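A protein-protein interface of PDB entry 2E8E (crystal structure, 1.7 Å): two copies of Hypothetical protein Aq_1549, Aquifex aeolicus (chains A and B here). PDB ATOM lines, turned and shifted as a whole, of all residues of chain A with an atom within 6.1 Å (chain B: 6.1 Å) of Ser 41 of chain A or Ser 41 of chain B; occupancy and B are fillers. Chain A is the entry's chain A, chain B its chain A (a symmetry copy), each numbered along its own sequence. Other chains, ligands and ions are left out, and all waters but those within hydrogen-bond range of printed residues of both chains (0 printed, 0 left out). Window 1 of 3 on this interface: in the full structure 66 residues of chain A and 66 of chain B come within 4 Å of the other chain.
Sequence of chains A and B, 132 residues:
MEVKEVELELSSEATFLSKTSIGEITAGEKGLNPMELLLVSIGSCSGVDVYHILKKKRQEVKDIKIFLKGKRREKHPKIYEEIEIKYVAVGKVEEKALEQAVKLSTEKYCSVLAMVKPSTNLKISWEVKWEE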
ATOM      1  N   ASN A  33     -28.270 -14.360 -13.732  1.00  0.00           N
ATOM      2  CA  ASN A  33     -28.354 -13.849 -15.096  1.00  0.00           C
ATOM      3  C   ASN A  33     -28.390 -12.319 -15.075  1.00  0.00           C
ATOM      4  O   ASN A  33     -29.223 -11.730 -14.398  1.00  0.00           O
ATOM      5  CB  ASN A  33     -29.602 -14.404 -15.783  1.00  0.00           C
ATOM      6  CG  ASN A  33     -29.788 -13.852 -17.170  1.00  0.00           C
ATOM      7  OD1 ASN A  33     -30.531 -12.889 -17.376  1.00  0.00           O
ATOM      8  ND2 ASN A  33     -29.086 -14.441 -18.138  1.00  0.00           N
ATOM      9  N   PRO A  34     -27.483 -11.658 -15.816  1.00  0.00           N
ATOM     10  CA  PRO A  34     -27.444 -10.187 -15.843  1.00  0.00           C
ATOM     11  C   PRO A  34     -28.761  -9.482 -16.172  1.00  0.00           C
ATOM     12  O   PRO A  34     -29.122  -8.502 -15.519  1.00  0.00           O
ATOM     13  CB  PRO A  34     -26.350  -9.891 -16.865  1.00  0.00           C
ATOM     14  CG  PRO A  34     -25.403 -11.051 -16.665  1.00  0.00           C
ATOM     15  CD  PRO A  34     -26.363 -12.224 -16.590  1.00  0.00           C
ATOM     16  N   MET A  35     -29.476  -9.963 -17.180  1.00  0.00           N
ATOM     17  CA  MET A  35     -30.737  -9.337 -17.545  1.00  0.00           C
ATOM     18  C   MET A  35     -31.821  -9.599 -16.500  1.00  0.00           C
ATOM     19  O   MET A  35     -32.721  -8.778 -16.318  1.00  0.00           O
ATOM     20  CB  MET A  35     -31.166  -9.782 -18.941  1.00  0.00           C
ATOM     21  CG  MET A  35     -30.463  -8.969 -20.048  1.00  0.00           C
ATOM     22  SD  MET A  35     -31.048  -7.241 -20.228  1.00  0.00           S
ATOM     23  CE  MET A  35     -32.328  -7.523 -21.446  1.00  0.00           C
ATOM     24  N   GLU A  36     -31.744 -10.733 -15.807  1.00  0.00           N
ATOM     25  CA  GLU A  36     -32.711 -10.986 -14.744  1.00  0.00           C
ATOM     26  C   GLU A  36     -32.362 -10.030 -13.605  1.00  0.00           C
ATOM     27  O   GLU A  36     -33.252  -9.502 -12.930  1.00  0.00           O
ATOM     28  CB  GLU A  36     -32.652 -12.442 -14.258  1.00  0.00           C
ATOM     29  CG  GLU A  36     -33.343 -13.415 -15.196  1.00  0.00           C
ATOM     30  CD  GLU A  36     -33.348 -14.846 -14.685  1.00  0.00           C
ATOM     31  OE1 GLU A  36     -32.832 -15.099 -13.573  1.00  0.00           O
ATOM     32  OE2 GLU A  36     -33.870 -15.720 -15.406  1.00  0.00           O
ATOM     33  N   LEU A  37     -31.065  -9.793 -13.395  1.00  0.00           N
ATOM     34  CA  LEU A  37     -30.631  -8.874 -12.344  1.00  0.00           C
ATOM     35  C   LEU A  37     -31.105  -7.450 -12.629  1.00  0.00           C
ATOM     36  O   LEU A  37     -31.361  -6.682 -11.701  1.00  0.00           O
ATOM     37  CB  LEU A  37     -29.104  -8.897 -12.181  1.00  0.00           C
ATOM     38  CG  LEU A  37     -28.565 -10.112 -11.421  1.00  0.00           C
ATOM     39  CD1 LEU A  37     -27.053 -10.004 -11.274  1.00  0.00           C
ATOM     40  CD2 LEU A  37     -29.227 -10.176 -10.041  1.00  0.00           C
ATOM     41  N   LEU A  38     -31.225  -7.090 -13.904  1.00  0.00           N
ATOM     42  CA  LEU A  38     -31.717  -5.753 -14.226  1.00  0.00           C
ATOM     43  C   LEU A  38     -33.164  -5.651 -13.738  1.00  0.00           C
ATOM     44  O   LEU A  38     -33.567  -4.636 -13.165  1.00  0.00           O
ATOM     45  CB  LEU A  38     -31.653  -5.483 -15.739  1.00  0.00           C
ATOM     46  CG  LEU A  38     -32.361  -4.193 -16.189  1.00  0.00           C
ATOM     47  CD1 LEU A  38     -31.732  -2.993 -15.479  1.00  0.00           C
ATOM     48  CD2 LEU A  38     -32.254  -4.028 -17.698  1.00  0.00           C
ATOM     49  N   LEU A  39     -33.948  -6.703 -13.963  1.00  0.00           N
ATOM     50  CA  LEU A  39     -35.339  -6.682 -13.515  1.00  0.00           C
ATOM     51  C   LEU A  39     -35.383  -6.618 -11.988  1.00  0.00           C
ATOM     52  O   LEU A  39     -36.247  -5.955 -11.410  1.00  0.00           O
ATOM     53  CB  LEU A  39     -36.096  -7.915 -14.017  1.00  0.00           C
ATOM     54  CG  LEU A  39     -36.325  -7.997 -15.530  1.00  0.00           C
ATOM     55  CD1 LEU A  39     -37.067  -9.283 -15.848  1.00  0.00           C
ATOM     56  CD2 LEU A  39     -37.136  -6.793 -16.016  1.00  0.00           C
ATOM     57  N   VAL A  40     -34.457  -7.304 -11.327  1.00  0.00           N
ATOM     58  CA  VAL A  40     -34.425  -7.258  -9.869  1.00  0.00           C
ATOM     59  C   VAL A  40     -34.095  -5.836  -9.410  1.00  0.00           C
ATOM     60  O   VAL A  40     -34.685  -5.335  -8.448  1.00  0.00           O
ATOM     61  CB  VAL A  40     -33.376  -8.248  -9.281  1.00  0.00           C
ATOM     62  CG1 VAL A  40     -33.195  -7.997  -7.785  1.00  0.00           C
ATOM     63  CG2 VAL A  40     -33.829  -9.681  -9.513  1.00  0.00           C
ATOM     64  N   SER A  41     -33.161  -5.182 -10.099  1.00  0.00           N
ATOM     65  CA  SER A  41     -32.777  -3.816  -9.740  1.00  0.00           C
ATOM     66  C   SER A  41     -33.970  -2.875  -9.877  1.00  0.00           C
ATOM     67  O   SER A  41     -34.225  -2.037  -9.011  1.00  0.00           O
ATOM     68  CB  SER A  41     -31.630  -3.332 -10.636  1.00  0.00           C
ATOM     69  OG  SER A  41     -30.510  -4.188 -10.501  1.00  0.00           O
ATOM     70  N   ILE A  42     -34.697  -3.020 -10.977  1.00  0.00           N
ATOM     71  CA  ILE A  42     -35.873  -2.198 -11.227  1.00  0.00           C
ATOM     72  C   ILE A  42     -36.938  -2.450 -10.161  1.00  0.00           C
ATOM     73  O   ILE A  42     -37.456  -1.511  -9.546  1.00  0.00           O
ATOM     74  CB  ILE A  42     -36.482  -2.521 -12.613  1.00  0.00           C
ATOM     75  CG1 ILE A  42     -35.529  -2.063 -13.725  1.00  0.00           C
ATOM     76  CG2 ILE A  42     -37.849  -1.864 -12.751  1.00  0.00           C
ATOM     77  CD1 ILE A  42     -35.940  -2.556 -15.115  1.00  0.00           C
ATOM     78  N   GLY A  43     -37.258  -3.726  -9.953  1.00  0.00           N
ATOM     79  CA  GLY A  43     -38.276  -4.102  -8.989  1.00  0.00           C
ATOM     80  C   GLY A  43     -37.986  -3.681  -7.564  1.00  0.00           C
ATOM     81  O   GLY A  43     -38.873  -3.176  -6.869  1.00  0.00           O
ATOM     82  N   SER A  44     -36.745  -3.871  -7.120  1.00  0.00           N
ATOM     83  CA  SER A  44     -36.388  -3.508  -5.757  1.00  0.00           C
ATOM     84  C   SER A  44     -36.296  -1.999  -5.568  1.00  0.00           C
ATOM     85  O   SER A  44     -36.715  -1.476  -4.532  1.00  0.00           O
ATOM     86  CB  SER A  44     -35.074  -4.188  -5.344  1.00  0.00           C
ATOM     87  OG  SER A  44     -34.009  -3.845  -6.214  1.00  0.00           O
ATOM     88  N   CYS A  45     -35.761  -1.290  -6.561  1.00  0.00           N
ATOM     89  CA  CYS A  45     -35.656   0.164  -6.460  1.00  0.00           C
ATOM     90  C   CYS A  45     -37.064   0.737  -6.305  1.00  0.00           C
ATOM     91  O   CYS A  45     -37.318   1.556  -5.421  1.00  0.00           O
ATOM     92  CB  CYS A  45     -35.005   0.753  -7.713  1.00  0.00           C
ATOM     93  SG  CYS A  45     -34.630   2.530  -7.599  1.00  0.00           S
ATOM     94  N   SER A  46     -37.979   0.290  -7.159  1.00  0.00           N
ATOM     95  CA  SER A  46     -39.363   0.769  -7.102  1.00  0.00           C
ATOM     96  C   SER A  46     -40.056   0.289  -5.829  1.00  0.00           C
ATOM     97  O   SER A  46     -40.815   1.038  -5.201  1.00  0.00           O
ATOM     98  CB  SER A  46     -40.144   0.279  -8.325  1.00  0.00           C
ATOM     99  OG  SER A  46     -41.473   0.791  -8.319  1.00  0.00           O
ATOM    100  N   CYS A 110     -38.242   6.337  -8.719  1.00  0.00           N
ATOM    101  CA  CYS A 110     -37.433   5.191  -9.127  1.00  0.00           C
ATOM    102  C   CYS A 110     -36.300   5.525 -10.091  1.00  0.00           C
ATOM    103  O   CYS A 110     -36.524   5.730 -11.287  1.00  0.00           O
ATOM    104  CB  CYS A 110     -38.321   4.113  -9.736  1.00  0.00           C
ATOM    105  SG  CYS A 110     -37.451   2.535  -9.911  1.00  0.00           S
ATOM    106  N   VAL A 112     -33.599   3.563 -11.080  1.00  0.00           N
ATOM    107  CA  VAL A 112     -33.290   2.508 -12.044  1.00  0.00           C
ATOM    108  C   VAL A 112     -34.279   2.517 -13.209  1.00  0.00           C
ATOM    109  O   VAL A 112     -33.883   2.506 -14.374  1.00  0.00           O
ATOM    110  CB  VAL A 112     -33.308   1.106 -11.374  1.00  0.00           C
ATOM    111  CG1 VAL A 112     -33.032   0.024 -12.417  1.00  0.00           C
ATOM    112  CG2 VAL A 112     -32.269   1.044 -10.251  1.00  0.00           C
ATOM    113  N   ASN B  33     -28.029  -2.938  -2.528  1.00  0.00           N
ATOM    114  CA  ASN B  33     -28.547  -1.652  -2.983  1.00  0.00           C
ATOM    115  C   ASN B  33     -28.987  -1.759  -4.444  1.00  0.00           C
ATOM    116  O   ASN B  33     -28.211  -2.177  -5.294  1.00  0.00           O
ATOM    117  CB  ASN B  33     -27.473  -0.575  -2.824  1.00  0.00           C
ATOM    118  CG  ASN B  33     -27.920   0.762  -3.349  1.00  0.00           C
ATOM    119  OD1 ASN B  33     -27.622   1.129  -4.489  1.00  0.00           O
ATOM    120  ND2 ASN B  33     -28.670   1.497  -2.529  1.00  0.00           N
ATOM    121  N   PRO B  34     -30.241  -1.382  -4.752  1.00  0.00           N
ATOM    122  CA  PRO B  34     -30.745  -1.464  -6.133  1.00  0.00           C
ATOM    123  C   PRO B  34     -29.892  -0.784  -7.206  1.00  0.00           C
ATOM    124  O   PRO B  34     -29.669  -1.352  -8.275  1.00  0.00           O
ATOM    125  CB  PRO B  34     -32.141  -0.857  -6.025  1.00  0.00           C
ATOM    126  CG  PRO B  34     -32.562  -1.269  -4.634  1.00  0.00           C
ATOM    127  CD  PRO B  34     -31.312  -0.964  -3.830  1.00  0.00           C
ATOM    128  N   MET B  35     -29.421   0.425  -6.935  1.00  0.00           N
ATOM    129  CA  MET B  35     -28.603   1.126  -7.913  1.00  0.00           C
ATOM    130  C   MET B  35     -27.219   0.492  -8.051  1.00  0.00           C
ATOM    131  O   MET B  35     -26.613   0.550  -9.122  1.00  0.00           O
ATOM    132  CB  MET B  35     -28.523   2.612  -7.571  1.00  0.00           C
ATOM    133  CG  MET B  35     -29.757   3.389  -8.073  1.00  0.00           C
ATOM    134  SD  MET B  35     -29.832   3.632  -9.888  1.00  0.00           S
ATOM    135  CE  MET B  35     -28.984   5.205  -9.977  1.00  0.00           C
ATOM    136  N   GLU B  36     -26.713  -0.116  -6.980  1.00  0.00           N
ATOM    137  CA  GLU B  36     -25.432  -0.804  -7.091  1.00  0.00           C
ATOM    138  C   GLU B  36     -25.682  -2.054  -7.932  1.00  0.00           C
ATOM    139  O   GLU B  36     -24.836  -2.448  -8.743  1.00  0.00           O
ATOM    140  CB  GLU B  36     -24.875  -1.190  -5.713  1.00  0.00           C
ATOM    141  CG  GLU B  36     -24.248  -0.022  -4.971  1.00  0.00           C
ATOM    142  CD  GLU B  36     -23.634  -0.414  -3.638  1.00  0.00           C
ATOM    143  OE1 GLU B  36     -23.664  -1.613  -3.280  1.00  0.00           O
ATOM    144  OE2 GLU B  36     -23.121   0.489  -2.946  1.00  0.00           O
ATOM    145  N   LEU B  37     -26.851  -2.674  -7.755  1.00  0.00           N
ATOM    146  CA  LEU B  37     -27.194  -3.864  -8.531  1.00  0.00           C
ATOM    147  C   LEU B  37     -27.306  -3.537 -10.019  1.00  0.00           C
ATOM    148  O   LEU B  37     -27.024  -4.385 -10.866  1.00  0.00           O
ATOM    149  CB  LEU B  37     -28.503  -4.495  -8.032  1.00  0.00           C
ATOM    150  CG  LEU B  37     -28.363  -5.307  -6.741  1.00  0.00           C
ATOM    151  CD1 LEU B  37     -29.704  -5.927  -6.370  1.00  0.00           C
ATOM    152  CD2 LEU B  37     -27.313  -6.403  -6.946  1.00  0.00           C
ATOM    153  N   LEU B  38     -27.715  -2.314 -10.346  1.00  0.00           N
ATOM    154  CA  LEU B  38     -27.796  -1.941 -11.756  1.00  0.00           C
ATOM    155  C   LEU B  38     -26.378  -1.956 -12.331  1.00  0.00           C
ATOM    156  O   LEU B  38     -26.154  -2.438 -13.444  1.00  0.00           O
ATOM    157  CB  LEU B  38     -28.418  -0.544 -11.930  1.00  0.00           C
ATOM    158  CG  LEU B  38     -28.331   0.021 -13.358  1.00  0.00           C
ATOM    159  CD1 LEU B  38     -29.045  -0.924 -14.325  1.00  0.00           C
ATOM    160  CD2 LEU B  38     -28.957   1.408 -13.419  1.00  0.00           C
ATOM    161  N   LEU B  39     -25.418  -1.430 -11.574  1.00  0.00           N
ATOM    162  CA  LEU B  39     -24.038  -1.421 -12.053  1.00  0.00           C
ATOM    163  C   LEU B  39     -23.534  -2.857 -12.190  1.00  0.00           C
ATOM    164  O   LEU B  39     -22.785  -3.177 -13.116  1.00  0.00           O
ATOM    165  CB  LEU B  39     -23.133  -0.628 -11.104  1.00  0.00           C
ATOM    166  CG  LEU B  39     -23.382   0.882 -11.037  1.00  0.00           C
ATOM    167  CD1 LEU B  39     -22.416   1.498 -10.041  1.00  0.00           C
ATOM    168  CD2 LEU B  39     -23.187   1.520 -12.415  1.00  0.00           C
ATOM    169  N   VAL B  40     -23.939  -3.730 -11.273  1.00  0.00           N
ATOM    170  CA  VAL B  40     -23.520  -5.124 -11.366  1.00  0.00           C
ATOM    171  C   VAL B  40     -24.114  -5.754 -12.627  1.00  0.00           C
ATOM    172  O   VAL B  40     -23.438  -6.513 -13.329  1.00  0.00           O
ATOM    173  CB  VAL B  40     -23.962  -5.947 -10.120  1.00  0.00           C
ATOM    174  CG1 VAL B  40     -23.728  -7.437 -10.361  1.00  0.00           C
ATOM    175  CG2 VAL B  40     -23.181  -5.493  -8.897  1.00  0.00           C
ATOM    176  N   SER B  41     -25.374  -5.435 -12.923  1.00  0.00           N
ATOM    177  CA  SER B  41     -26.032  -5.983 -14.110  1.00  0.00           C
ATOM    178  C   SER B  41     -25.302  -5.540 -15.375  1.00  0.00           C
ATOM    179  O   SER B  41     -25.062  -6.334 -16.285  1.00  0.00           O
ATOM    180  CB  SER B  41     -27.494  -5.524 -14.169  1.00  0.00           C
ATOM    181  OG  SER B  41     -28.186  -5.947 -13.008  1.00  0.00           O
ATOM    182  N   ILE B  42     -24.955  -4.260 -15.423  1.00  0.00           N
ATOM    183  CA  ILE B  42     -24.239  -3.707 -16.564  1.00  0.00           C
ATOM    184  C   ILE B  42     -22.868  -4.368 -16.707  1.00  0.00           C
ATOM    185  O   ILE B  42     -22.503  -4.848 -17.786  1.00  0.00           O
ATOM    186  CB  ILE B  42     -24.032  -2.183 -16.394  1.00  0.00           C
ATOM    187  CG1 ILE B  42     -25.380  -1.457 -16.481  1.00  0.00           C
ATOM    188  CG2 ILE B  42     -23.057  -1.666 -17.445  1.00  0.00           C
ATOM    189  CD1 ILE B  42     -25.299   0.020 -16.087  1.00  0.00           C
ATOM    190  N   GLY B  43     -22.116  -4.383 -15.607  1.00  0.00           N
ATOM    191  CA  GLY B  43     -20.781  -4.953 -15.614  1.00  0.00           C
ATOM    192  C   GLY B  43     -20.721  -6.422 -15.979  1.00  0.00           C
ATOM    193  O   GLY B  43     -19.864  -6.835 -16.767  1.00  0.00           O
ATOM    194  N   SER B  44     -21.632  -7.218 -15.423  1.00  0.00           N
ATOM    195  CA  SER B  44     -21.633  -8.646 -15.709  1.00  0.00           C
ATOM    196  C   SER B  44     -22.128  -8.950 -17.118  1.00  0.00           C
ATOM    197  O   SER B  44     -21.588  -9.834 -17.789  1.00  0.00           O
ATOM    198  CB  SER B  44     -22.465  -9.404 -14.666  1.00  0.00           C
ATOM    199  OG  SER B  44     -23.802  -8.936 -14.618  1.00  0.00           O
ATOM    200  N   CYS B  45     -23.144  -8.222 -17.579  1.00  0.00           N
ATOM    201  CA  CYS B  45     -23.661  -8.444 -18.929  1.00  0.00           C
ATOM    202  C   CYS B  45     -22.532  -8.186 -19.924  1.00  0.00           C
ATOM    203  O   CYS B  45     -22.280  -8.997 -20.817  1.00  0.00           O
ATOM    204  CB  CYS B  45     -24.826  -7.497 -19.229  1.00  0.00           C
ATOM    205  SG  CYS B  45     -25.682  -7.837 -20.798  1.00  0.00           S
ATOM    206  N   SER B  46     -21.843  -7.061 -19.756  1.00  0.00           N
ATOM    207  CA  SER B  46     -20.736  -6.712 -20.651  1.00  0.00           C
ATOM    208  C   SER B  46     -19.561  -7.671 -20.468  1.00  0.00           C
ATOM    209  O   SER B  46     -18.918  -8.076 -21.443  1.00  0.00           O
ATOM    210  CB  SER B  46     -20.271  -5.278 -20.384  1.00  0.00           C
ATOM    211  OG  SER B  46     -19.239  -4.899 -21.291  1.00  0.00           O
ATOM    212  N   CYS B 110     -23.996  -5.888 -25.505  1.00  0.00           N
ATOM    213  CA  CYS B 110     -24.491  -5.681 -24.146  1.00  0.00           C
ATOM    214  C   CYS B 110     -25.915  -5.144 -24.064  1.00  0.00           C
ATOM    215  O   CYS B 110     -26.158  -3.953 -24.280  1.00  0.00           O
ATOM    216  CB  CYS B 110     -23.551  -4.757 -23.381  1.00  0.00           C
ATOM    217  SG  CYS B 110     -23.891  -4.762 -21.603  1.00  0.00           S
ATOM    218  N   VAL B 112     -28.032  -4.927 -21.308  1.00  0.00           N
ATOM    219  CA  VAL B 112     -28.284  -4.043 -20.171  1.00  0.00           C
ATOM    220  C   VAL B 112     -27.771  -2.630 -20.445  1.00  0.00           C
ATOM    221  O   VAL B 112     -28.492  -1.649 -20.262  1.00  0.00           O
ATOM    222  CB  VAL B 112     -27.616  -4.583 -18.876  1.00  0.00           C
ATOM    223  CG1 VAL B 112     -27.855  -3.612 -17.721  1.00  0.00           C
ATOM    224  CG2 VAL B 112     -28.171  -5.969 -18.534  1.00  0.00           C
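Of the 16 printed residues of chain B, 8 touch a printed residue of chain A. Of the 16 printed residues of chain A, 8 touch a printed residue of chain B. Hydrophobic or aromatic side chains of chain A within 4 Å of the printed part of chain B: Pro 34, Met 35, Leu 37, Leu 38 and Val 112. Among the printed residues, 14 pairs touch across the chains.
The side-chain hydroxyl of Ser 44 of chain A lies within hydrogen-bond range of the backbone carbonyl oxygen of Val 40 of chain A. The side-chain amide oxygen of Asn 33 of chain A lies within hydrogen-bond range of the backbone NH of Met 35 of chain A, 3.1 Å away. The side-chain hydroxyl (OG) of Ser 44 of chain B lies within hydrogen-bond range of the backbone carbonyl oxygen (O) of Ser 41 of chain B (3.3 Å). O of Leu 37 of chain B is in hydrogen-bond range of OG of Ser 41 of chain B (2.9 Å). The side-chain sulfur (SG) of Cys 45 of chain B lies within hydrogen-bond range of the side-chain sulfur (SG) of Cys 110 of chain B. SG of Cys 45 of chain A sits at hydrogen-bond distance from SG of Cys 110 of chain A (3.6 Å).
Ser 41 of chain A touches four residues of chain B. Of the printed residues of chain B, Cys 45 of chain A touches Pro 34. Cys 110 of chain A touches none of the printed residues of chain B. Glu 36 of chain B touches none of the printed residues of chain A. Of the printed residues of chain A, Leu 38 of chain B touches Leu 38 (3.6 Å) and Ser 41 (3.4 Å). Ser 41 of chain B touches four residues of chain A. The nearest residue of chain A that does not touch Ser 41 of chain B is Met 35 of chain A (5.7 Å). The nearest printed residue of chain B that does not touch Pro 34 of chain A is Val 112 of chain B (4.1 Å).
Met 35 of chain A touches Val 112 of chain B, and with the chains exchanged Val 112 of chain A touches Met 35 of chain B. Leu 38 of chain A touches its own counterpart, Leu 38 of chain B. Leu 38 of chain A touches Ser 41 of chain B, and with the chains exchanged Ser 41 of chain A touches Leu 38 of chain B. Ser 41 of chain A touches its own counterpart, Ser 41 of chain B. Positions printed for both chains: 33, 34, 35, 36, 37, 38, 39, 40, 41, 42, 43, 44, 45, 46, 110 and 112.
Ser 41 of chain B touches Pro 34 of chain A (CB to O, 3.7 Å). CG of Pro 34 of chain A touches OG of Ser 44 of chain B (3.4 Å). Pro 34 of chain A touches Cys 45 of chain B (CB to N, 3.7 Å). Met 35 of chain A touches Val 112 of chain B (SD to CG2, 3.6 Å). Leu 37 of chain A touches Ser 41 of chain B (CB to OG, 3.2 Å). CD1 of Leu 38 of chain B touches CD1 of Leu 38 of chain A, at 3.6 Å. Ser 41 of chain A touches Leu 37 of chain B. Ser 41 of chain A touches Ser 41 of chain B. Cys 45 of chain A touches Pro 34 of chain B (N to CB, 3.7 Å). Met 35 of chain B touches Val 112 of chain A (SD to CG2, 3.6 Å).
OG of Ser 41 of chain A lies within hydrogen-bond range of N of Leu 38 of chain B, 3.4 Å away. The backbone NH (N) of Leu 38 of chain A lies within hydrogen-bond range of the side-chain hydroxyl (OG) of Ser 41 of chain B.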
